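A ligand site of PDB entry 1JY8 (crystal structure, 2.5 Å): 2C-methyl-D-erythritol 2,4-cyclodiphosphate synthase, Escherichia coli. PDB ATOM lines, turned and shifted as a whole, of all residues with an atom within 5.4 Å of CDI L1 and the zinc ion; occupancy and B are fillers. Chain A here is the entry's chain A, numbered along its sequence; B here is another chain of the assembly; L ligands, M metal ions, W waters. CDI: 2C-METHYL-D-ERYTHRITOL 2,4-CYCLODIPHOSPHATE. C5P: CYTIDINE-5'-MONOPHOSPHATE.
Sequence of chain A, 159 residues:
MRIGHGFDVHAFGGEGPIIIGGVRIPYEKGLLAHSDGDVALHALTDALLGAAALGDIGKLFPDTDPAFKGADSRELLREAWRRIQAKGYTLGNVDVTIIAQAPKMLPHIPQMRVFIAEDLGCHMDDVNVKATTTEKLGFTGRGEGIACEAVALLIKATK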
ATOM      1  N   ASP A   8      27.215   2.321 -23.303  1.00  0.00           N
ATOM      2  CA  ASP A   8      26.221   2.600 -22.260  1.00  0.00           C
ATOM      3  C   ASP A   8      26.509   1.783 -20.993  1.00  0.00           C
ATOM      4  O   ASP A   8      27.197   0.743 -21.040  1.00  0.00           O
ATOM      5  CB  ASP A   8      24.816   2.300 -22.776  1.00  0.00           C
ATOM      6  CG  ASP A   8      23.729   2.902 -21.895  1.00  0.00           C
ATOM      7  OD1 ASP A   8      22.596   2.390 -21.940  1.00  0.00           O
ATOM      8  OD2 ASP A   8      23.987   3.869 -21.139  1.00  0.00           O
ATOM      9  N   VAL A   9      26.015   2.288 -19.859  1.00  0.00           N
ATOM     10  CA  VAL A   9      26.186   1.653 -18.550  1.00  0.00           C
ATOM     11  C   VAL A   9      24.922   1.862 -17.715  1.00  0.00           C
ATOM     12  O   VAL A   9      24.262   2.906 -17.834  1.00  0.00           O
ATOM     13  CB  VAL A   9      27.385   2.281 -17.756  1.00  0.00           C
ATOM     14  CG1 VAL A   9      27.399   1.796 -16.325  1.00  0.00           C
ATOM     15  CG2 VAL A   9      28.704   1.931 -18.395  1.00  0.00           C
ATOM     16  N   HIS A  10      24.541   0.834 -16.951  1.00  0.00           N
ATOM     17  CA  HIS A  10      23.390   0.896 -16.042  1.00  0.00           C
ATOM     18  C   HIS A  10      23.753   0.145 -14.773  1.00  0.00           C
ATOM     19  O   HIS A  10      24.456  -0.859 -14.805  1.00  0.00           O
ATOM     20  CB  HIS A  10      22.097   0.391 -16.674  1.00  0.00           C
ATOM     21  CG  HIS A  10      21.483   1.384 -17.609  1.00  0.00           C
ATOM     22  ND1 HIS A  10      21.023   2.612 -17.186  1.00  0.00           N
ATOM     23  CD2 HIS A  10      21.361   1.381 -18.961  1.00  0.00           C
ATOM     24  CE1 HIS A  10      20.652   3.321 -18.237  1.00  0.00           C
ATOM     25  NE2 HIS A  10      20.855   2.599 -19.328  1.00  0.00           N
ATOM     26  N   ALA A  33      17.146   2.344 -14.409  1.00  0.00           N
ATOM     27  CA  ALA A  33      17.124   3.232 -15.578  1.00  0.00           C
ATOM     28  C   ALA A  33      15.744   3.853 -15.782  1.00  0.00           C
ATOM     29  O   ALA A  33      14.773   3.404 -15.178  1.00  0.00           O
ATOM     30  CB  ALA A  33      17.540   2.455 -16.830  1.00  0.00           C
ATOM     31  N   HIS A  34      15.678   4.909 -16.598  1.00  0.00           N
ATOM     32  CA  HIS A  34      14.412   5.590 -16.915  1.00  0.00           C
ATOM     33  C   HIS A  34      13.493   4.621 -17.659  1.00  0.00           C
ATOM     34  O   HIS A  34      12.303   4.509 -17.344  1.00  0.00           O
ATOM     35  CB  HIS A  34      14.674   6.831 -17.776  1.00  0.00           C
ATOM     36  CG  HIS A  34      13.451   7.656 -18.050  1.00  0.00           C
ATOM     37  ND1 HIS A  34      12.552   8.025 -17.066  1.00  0.00           N
ATOM     38  CD2 HIS A  34      12.997   8.229 -19.198  1.00  0.00           C
ATOM     39  CE1 HIS A  34      11.601   8.782 -17.592  1.00  0.00           C
ATOM     40  NE2 HIS A  34      11.854   8.920 -18.884  1.00  0.00           N
ATOM     41  N   SER A  35      14.038   3.976 -18.690  1.00  0.00           N
ATOM     42  CA  SER A  35      13.333   2.998 -19.515  1.00  0.00           C
ATOM     43  C   SER A  35      13.547   1.651 -18.828  1.00  0.00           C
ATOM     44  O   SER A  35      13.803   1.601 -17.628  1.00  0.00           O
ATOM     45  CB  SER A  35      13.957   2.968 -20.922  1.00  0.00           C
ATOM     46  OG  SER A  35      15.264   2.419 -20.915  1.00  0.00           O
ATOM     47  N   ASP A  36      13.477   0.558 -19.589  1.00  0.00           N
ATOM     48  CA  ASP A  36      13.701  -0.776 -19.037  1.00  0.00           C
ATOM     49  C   ASP A  36      15.199  -1.006 -18.730  1.00  0.00           C
ATOM     50  O   ASP A  36      15.573  -2.078 -18.260  1.00  0.00           O
ATOM     51  CB  ASP A  36      13.195  -1.858 -19.996  1.00  0.00           C
ATOM     52  CG  ASP A  36      13.816  -1.754 -21.366  1.00  0.00           C
ATOM     53  OD1 ASP A  36      13.386  -2.506 -22.262  1.00  0.00           O
ATOM     54  OD2 ASP A  36      14.726  -0.924 -21.563  1.00  0.00           O
ATOM     55  N   GLY A  37      16.034  -0.021 -19.063  1.00  0.00           N
ATOM     56  CA  GLY A  37      17.455  -0.091 -18.787  1.00  0.00           C
ATOM     57  C   GLY A  37      18.278  -1.050 -19.623  1.00  0.00           C
ATOM     58  O   GLY A  37      19.397  -1.401 -19.237  1.00  0.00           O
ATOM     59  N   ASP A  38      17.767  -1.429 -20.783  1.00  0.00           N
ATOM     60  CA  ASP A  38      18.478  -2.346 -21.661  1.00  0.00           C
ATOM     61  C   ASP A  38      19.790  -1.724 -22.167  1.00  0.00           C
ATOM     62  O   ASP A  38      19.808  -1.005 -23.167  1.00  0.00           O
ATOM     63  CB  ASP A  38      17.577  -2.729 -22.826  1.00  0.00           C
ATOM     64  CG  ASP A  38      18.045  -3.936 -23.564  1.00  0.00           C
ATOM     65  OD1 ASP A  38      19.270  -4.076 -23.765  1.00  0.00           O
ATOM     66  OD2 ASP A  38      17.195  -4.738 -23.973  1.00  0.00           O
ATOM     67  N   VAL A  39      20.885  -2.012 -21.478  1.00  0.00           N
ATOM     68  CA  VAL A  39      22.195  -1.460 -21.820  1.00  0.00           C
ATOM     69  C   VAL A  39      22.652  -1.795 -23.240  1.00  0.00           C
ATOM     70  O   VAL A  39      23.312  -0.980 -23.887  1.00  0.00           O
ATOM     71  CB  VAL A  39      23.309  -1.962 -20.882  1.00  0.00           C
ATOM     72  CG1 VAL A  39      24.409  -0.934 -20.798  1.00  0.00           C
ATOM     73  CG2 VAL A  39      22.772  -2.246 -19.528  1.00  0.00           C
ATOM     74  N   HIS A  42      20.564   0.245 -25.934  1.00  0.00           N
ATOM     75  CA  HIS A  42      20.879   1.671 -25.866  1.00  0.00           C
ATOM     76  C   HIS A  42      22.203   1.892 -26.599  1.00  0.00           C
ATOM     77  O   HIS A  42      22.305   2.740 -27.473  1.00  0.00           O
ATOM     78  CB  HIS A  42      21.046   2.160 -24.435  1.00  0.00           C
ATOM     79  CG  HIS A  42      19.764   2.204 -23.656  1.00  0.00           C
ATOM     80  ND1 HIS A  42      19.706   2.623 -22.338  1.00  0.00           N
ATOM     81  CD2 HIS A  42      18.502   1.888 -24.012  1.00  0.00           C
ATOM     82  CE1 HIS A  42      18.455   2.554 -21.919  1.00  0.00           C
ATOM     83  NE2 HIS A  42      17.699   2.111 -22.912  1.00  0.00           N
ATOM     84  N   ILE A  57      20.820   8.733 -28.237  1.00  0.00           N
ATOM     85  CA  ILE A  57      19.552   8.323 -27.643  1.00  0.00           C
ATOM     86  C   ILE A  57      18.928   9.333 -26.696  1.00  0.00           C
ATOM     87  O   ILE A  57      17.722   9.557 -26.744  1.00  0.00           O
ATOM     88  CB  ILE A  57      19.699   6.920 -26.959  1.00  0.00           C
ATOM     89  CG1 ILE A  57      18.351   6.258 -26.808  1.00  0.00           C
ATOM     90  CG2 ILE A  57      20.352   7.034 -25.591  1.00  0.00           C
ATOM     91  CD1 ILE A  57      18.465   4.867 -26.260  1.00  0.00           C
ATOM     92  N   GLY A  58      19.752   9.985 -25.880  1.00  0.00           N
ATOM     93  CA  GLY A  58      19.224  10.963 -24.936  1.00  0.00           C
ATOM     94  C   GLY A  58      18.644  12.179 -25.609  1.00  0.00           C
ATOM     95  O   GLY A  58      17.665  12.772 -25.146  1.00  0.00           O
ATOM     96  N   PHE A  61      15.244  10.793 -27.130  1.00  0.00           N
ATOM     97  CA  PHE A  61      14.302  10.322 -26.127  1.00  0.00           C
ATOM     98  C   PHE A  61      14.783  10.717 -24.720  1.00  0.00           C
ATOM     99  O   PHE A  61      15.282   9.886 -23.975  1.00  0.00           O
ATOM    100  CB  PHE A  61      14.147   8.790 -26.220  1.00  0.00           C
ATOM    101  CG  PHE A  61      14.098   8.270 -27.645  1.00  0.00           C
ATOM    102  CD1 PHE A  61      13.059   8.603 -28.498  1.00  0.00           C
ATOM    103  CD2 PHE A  61      15.124   7.453 -28.135  1.00  0.00           C
ATOM    104  CE1 PHE A  61      13.046   8.157 -29.825  1.00  0.00           C
ATOM    105  CE2 PHE A  61      15.118   7.002 -29.457  1.00  0.00           C
ATOM    106  CZ  PHE A  61      14.076   7.357 -30.304  1.00  0.00           C
ATOM    107  N   PRO A  62      14.584  11.984 -24.337  1.00  0.00           N
ATOM    108  CA  PRO A  62      14.963  12.577 -23.048  1.00  0.00           C
ATOM    109  C   PRO A  62      14.572  11.857 -21.747  1.00  0.00           C
ATOM    110  O   PRO A  62      13.426  11.475 -21.556  1.00  0.00           O
ATOM    111  CB  PRO A  62      14.305  13.954 -23.119  1.00  0.00           C
ATOM    112  CG  PRO A  62      14.386  14.278 -24.561  1.00  0.00           C
ATOM    113  CD  PRO A  62      13.930  12.992 -25.188  1.00  0.00           C
ATOM    114  N   ASP A  63      15.551  11.781 -20.838  1.00  0.00           N
ATOM    115  CA  ASP A  63      15.390  11.171 -19.507  1.00  0.00           C
ATOM    116  C   ASP A  63      14.285  11.857 -18.731  1.00  0.00           C
ATOM    117  O   ASP A  63      13.664  11.266 -17.846  1.00  0.00           O
ATOM    118  CB  ASP A  63      16.695  11.339 -18.698  1.00  0.00           C
ATOM    119  CG  ASP A  63      17.602  10.134 -18.791  1.00  0.00           C
ATOM    120  OD1 ASP A  63      17.512   9.360 -19.775  1.00  0.00           O
ATOM    121  OD2 ASP A  63      18.420   9.935 -17.861  1.00  0.00           O
ATOM    122  N   ASP A  65      11.486  13.442 -20.157  1.00  0.00           N
ATOM    123  CA  ASP A  65      10.186  13.152 -20.725  1.00  0.00           C
ATOM    124  C   ASP A  65       9.643  11.852 -20.122  1.00  0.00           C
ATOM    125  O   ASP A  65      10.188  10.768 -20.367  1.00  0.00           O
ATOM    126  CB  ASP A  65      10.294  13.033 -22.243  1.00  0.00           C
ATOM    127  CG  ASP A  65       8.944  13.035 -22.925  1.00  0.00           C
ATOM    128  OD1 ASP A  65       7.952  12.586 -22.312  1.00  0.00           O
ATOM    129  OD2 ASP A  65       8.875  13.504 -24.088  1.00  0.00           O
ATOM    130  N   PHE A  68       8.869   8.233 -21.718  1.00  0.00           N
ATOM    131  CA  PHE A  68       9.861   7.180 -21.872  1.00  0.00           C
ATOM    132  C   PHE A  68      10.131   6.416 -20.588  1.00  0.00           C
ATOM    133  O   PHE A  68      11.126   5.711 -20.491  1.00  0.00           O
ATOM    134  CB  PHE A  68      11.161   7.791 -22.412  1.00  0.00           C
ATOM    135  CG  PHE A  68      10.941   8.754 -23.533  1.00  0.00           C
ATOM    136  CD1 PHE A  68      11.408  10.056 -23.460  1.00  0.00           C
ATOM    137  CD2 PHE A  68      10.237   8.369 -24.673  1.00  0.00           C
ATOM    138  CE1 PHE A  68      11.194  10.960 -24.493  1.00  0.00           C
ATOM    139  CE2 PHE A  68      10.019   9.257 -25.717  1.00  0.00           C
ATOM    140  CZ  PHE A  68      10.488  10.560 -25.626  1.00  0.00           C
ATOM    141  N   SER A  73      13.020  -0.512 -24.654  1.00  0.00           N
ATOM    142  CA  SER A  73      14.146  -0.056 -25.455  1.00  0.00           C
ATOM    143  C   SER A  73      14.089  -0.518 -26.910  1.00  0.00           C
ATOM    144  O   SER A  73      14.760   0.054 -27.765  1.00  0.00           O
ATOM    145  CB  SER A  73      15.465  -0.440 -24.810  1.00  0.00           C
ATOM    146  OG  SER A  73      15.686   0.305 -23.625  1.00  0.00           O
ATOM    147  N   LEU A  76      12.300   2.134 -28.707  1.00  0.00           N
ATOM    148  CA  LEU A  76      13.226   3.235 -28.973  1.00  0.00           C
ATOM    149  C   LEU A  76      14.170   2.884 -30.113  1.00  0.00           C
ATOM    150  O   LEU A  76      14.523   3.729 -30.920  1.00  0.00           O
ATOM    151  CB  LEU A  76      14.034   3.567 -27.715  1.00  0.00           C
ATOM    152  CG  LEU A  76      13.282   4.004 -26.458  1.00  0.00           C
ATOM    153  CD1 LEU A  76      14.297   4.438 -25.394  1.00  0.00           C
ATOM    154  CD2 LEU A  76      12.353   5.160 -26.784  1.00  0.00           C
ATOM    155  N   THR B 132      27.465  10.167 -22.676  1.00  0.00           N
ATOM    156  CA  THR B 132      26.775   9.239 -21.790  1.00  0.00           C
ATOM    157  C   THR B 132      27.505   9.269 -20.451  1.00  0.00           C
ATOM    158  O   THR B 132      28.675   9.643 -20.395  1.00  0.00           O
ATOM    159  CB  THR B 132      26.749   7.798 -22.330  1.00  0.00           C
ATOM    160  OG1 THR B 132      25.856   7.007 -21.526  1.00  0.00           O
ATOM    161  CG2 THR B 132      28.140   7.160 -22.272  1.00  0.00           C
ATOM    162  N   GLU B 135      26.447   6.201 -14.989  1.00  0.00           N
ATOM    163  CA  GLU B 135      25.508   6.108 -13.858  1.00  0.00           C
ATOM    164  C   GLU B 135      26.170   6.088 -12.476  1.00  0.00           C
ATOM    165  O   GLU B 135      25.885   5.217 -11.652  1.00  0.00           O
ATOM    166  CB  GLU B 135      24.611   4.886 -14.034  1.00  0.00           C
ATOM    167  CG  GLU B 135      23.961   4.751 -15.407  1.00  0.00           C
ATOM    168  CD  GLU B 135      22.774   5.680 -15.630  1.00  0.00           C
ATOM    169  OE1 GLU B 135      22.262   5.754 -16.757  1.00  0.00           O
ATOM    170  OE2 GLU B 135      22.331   6.327 -14.656  1.00  0.00           O
HETATM  171  C4  CDI L   1      15.112   7.015 -22.097  1.00  0.00           C
HETATM  172  C3  CDI L   1      16.654   6.774 -22.125  1.00  0.00           C
HETATM  173  OB4 CDI L   1      17.110   6.647 -20.747  1.00  0.00           O
HETATM  174  PB  CDI L   1      17.667   5.540 -19.691  1.00  0.00           P
HETATM  175  OB2 CDI L   1      17.945   6.183 -18.277  1.00  0.00           O
HETATM  176  OB3 CDI L   1      16.655   4.293 -19.546  1.00  0.00           O
HETATM  177  PA  CDI L   1      20.124   6.280 -20.468  1.00  0.00           P
HETATM  178  OA3 CDI L   1      19.676   7.503 -21.422  1.00  0.00           O
HETATM  179  OA1 CDI L   1      20.769   6.791 -19.128  1.00  0.00           O
HETATM  180  OA2 CDI L   1      21.132   5.277 -21.188  1.00  0.00           O
HETATM  181  C1  CDI L   1      19.057   7.772 -22.718  1.00  0.00           C
HETATM  182  C2  CDI L   1      17.482   7.963 -22.714  1.00  0.00           C
HETATM  183  O1  CDI L   1      17.139   8.201 -24.079  1.00  0.00           O
HETATM  184  C5  CDI L   1      16.918   5.475 -22.950  1.00  0.00           C
HETATM  185  O2  CDI L   1      14.794   8.210 -21.357  1.00  0.00           O
HETATM  186  OB1 CDI L   1      19.168   5.255 -19.917  1.00  0.00           O
HETATM  187  O3P C5P L   2      22.468   7.818 -20.525  1.00  0.00           O
HETATM  188  P   C5P L   2      22.645   9.214 -19.633  1.00  0.00           P
HETATM  189  O1P C5P L   2      24.096   9.351 -19.181  1.00  0.00           O
HETATM  190  O2P C5P L   2      21.717   9.215 -18.408  1.00  0.00           O
HETATM  191  O5' C5P L   2      22.233  10.549 -20.549  1.00  0.00           O
HETATM  192  C5' C5P L   2      22.057  10.473 -21.957  1.00  0.00           C
HETATM  193  C4' C5P L   2      21.978  11.847 -22.490  1.00  0.00           C
HETATM  194  O4' C5P L   2      22.510  12.833 -21.618  1.00  0.00           O
HETATM  195  C3' C5P L   2      22.970  11.810 -23.662  1.00  0.00           C
HETATM  196  O3' C5P L   2      22.241  12.285 -24.750  1.00  0.00           O
HETATM  197  C2' C5P L   2      24.068  12.796 -23.327  1.00  0.00           C
HETATM  198  O2' C5P L   2      24.457  13.672 -24.400  1.00  0.00           O
HETATM  199  C1' C5P L   2      23.485  13.609 -22.221  1.00  0.00           C
HETATM  200  N1  C5P L   2      24.667  13.512 -21.484  1.00  0.00           N
HETATM  201  C2  C5P L   2      25.407  14.708 -21.604  1.00  0.00           C
HETATM  202  N3  C5P L   2      26.593  14.909 -20.952  1.00  0.00           N
HETATM  203  C4  C5P L   2      27.098  13.951 -20.163  1.00  0.00           C
HETATM  204  C5  C5P L   2      26.417  12.747 -20.013  1.00  0.00           C
HETATM  205  C6  C5P L   2      25.221  12.588 -20.689  1.00  0.00           C
HETATM  206  O2  C5P L   2      25.035  15.670 -22.297  1.00  0.00           O
HETATM  207  N4  C5P L   2      28.250  14.177 -19.536  1.00  0.00           N
HETATM  208 ZN    ZN M   1      21.111   3.333 -21.144  1.00  0.00          ZN
HETATM  209  O   HOH W   1      16.980   8.224 -16.047  1.00  0.00           O
HETATM  210  O   HOH W   2      24.001   5.803 -18.737  1.00  0.00           O
HETATM  211  O   HOH W   3      19.603   5.855 -16.363  1.00  0.00           O
HETATM  212  O   HOH W   4      23.443   6.492 -22.829  1.00  0.00           O
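The backbone carbonyl oxygen of Phe 61 is in hydrogen-bond range of an oxygen (O1) of CDI L1 (2.5 Å). N of Ser 35 sits at hydrogen-bond distance from OB3 of CDI L1 (2.8 Å). The side-chain hydroxyl (OG) of Ser 35 lies within hydrogen-bond range of an oxygen (OB3) of CDI L1 (2.7 Å). N of His 34 lies within hydrogen-bond range of OB2 of CDI L1, at 3.1 Å. The side-chain carboxylate of Asp 63 lies close to an oxygen (O2) of CDI L1 (3.3 Å). An oxygen (OA1) of CDI L1 sits close to the side-chain carboxylate (OE1) of Glu 135 of chain B (3.0 Å). The backbone carbonyl oxygen of Ile 57 is in hydrogen-bond range of an oxygen (O1) of CDI L1, at 3.0 Å.
An oxygen (OA2) of CDI L1 sits close to an oxygen (O3P) of C5P L2 (2.9 Å).
A ring nitrogen (ND1) of His 10 lies close to the side-chain carboxylate (OE1) of Glu 135 of chain B. The side-chain hydroxyl (OG) of Ser 35 lies within hydrogen-bond range of a ring nitrogen (NE2) of His 42 (3.2 Å). A ring nitrogen (NE2) of His 42 sits at hydrogen-bond distance from the side-chain hydroxyl (OG) of Ser 73, at 2.8 Å. The backbone NH of Gly 37 sits close to the side-chain hydroxyl of Ser 35 (3.2 Å). The side-chain hydroxyl (OG) of Ser 35 is in hydrogen-bond range of the side-chain carboxylate (OD2) of Asp 36 (3.4 Å). The side-chain hydroxyl of Ser 35 lies within hydrogen-bond range of the side-chain hydroxyl of Ser 73 (3.5 Å). The backbone carbonyl oxygen (O) of Asp 63 lies within hydrogen-bond range of a ring nitrogen (NE2) of His 34 (3.1 Å). A ring nitrogen (NE2) of His 34 is in hydrogen-bond range of the backbone carbonyl oxygen (O) of Asp 65 (2.9 Å).
Merely in contact with CDI L1: Ala 33 (3.4 Å), Pro 62 (3.5 Å), Gly 58 (3.6 Å), Leu 76 (3.7 Å) and Phe 68 (3.8 Å). Hydrophobic or aromatic side chains within 4 Å of CDI L1: His 10, Ala 33, His 34, His 42, Ile 57, Phe 61, Phe 68 and Leu 76. Of the 22 residues printed, 14 come within 4 Å of CDI L1. The nearest printed residue that does not touch CDI L1 is Gly 37 (4.4 Å).
Of the 22 residues printed, 3 come within 4 Å of the zinc ion. The nearest printed residue that does not touch the zinc ion is Val 9 (4.6 Å).
The zinc ion is bound by the side-chain carboxylate (OD1) of Asp 8 (1.9 Å). OA2 of CDI L1 binds the zinc ion. NE2 of His 10 binds the zinc ion (2.0 Å). The zinc ion is bound by ND1 of His 42 (2.0 Å).
Water W3 lies within hydrogen-bond range of OB2 of CDI L1 (2.6 Å) and OE1 of Glu 135 of chain B (2.7 Å). Water W4 lies within hydrogen-bond range of the side-chain hydroxyl (OG1) of Thr 132 of chain B, an oxygen (O3P) of C5P L2 and the side-chain carboxylate (OD2) of Asp 8. Water W1 lies within hydrogen-bond range of the side-chain carboxylate (OD2) of Asp 63 and an oxygen (OB2) of CDI L1.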
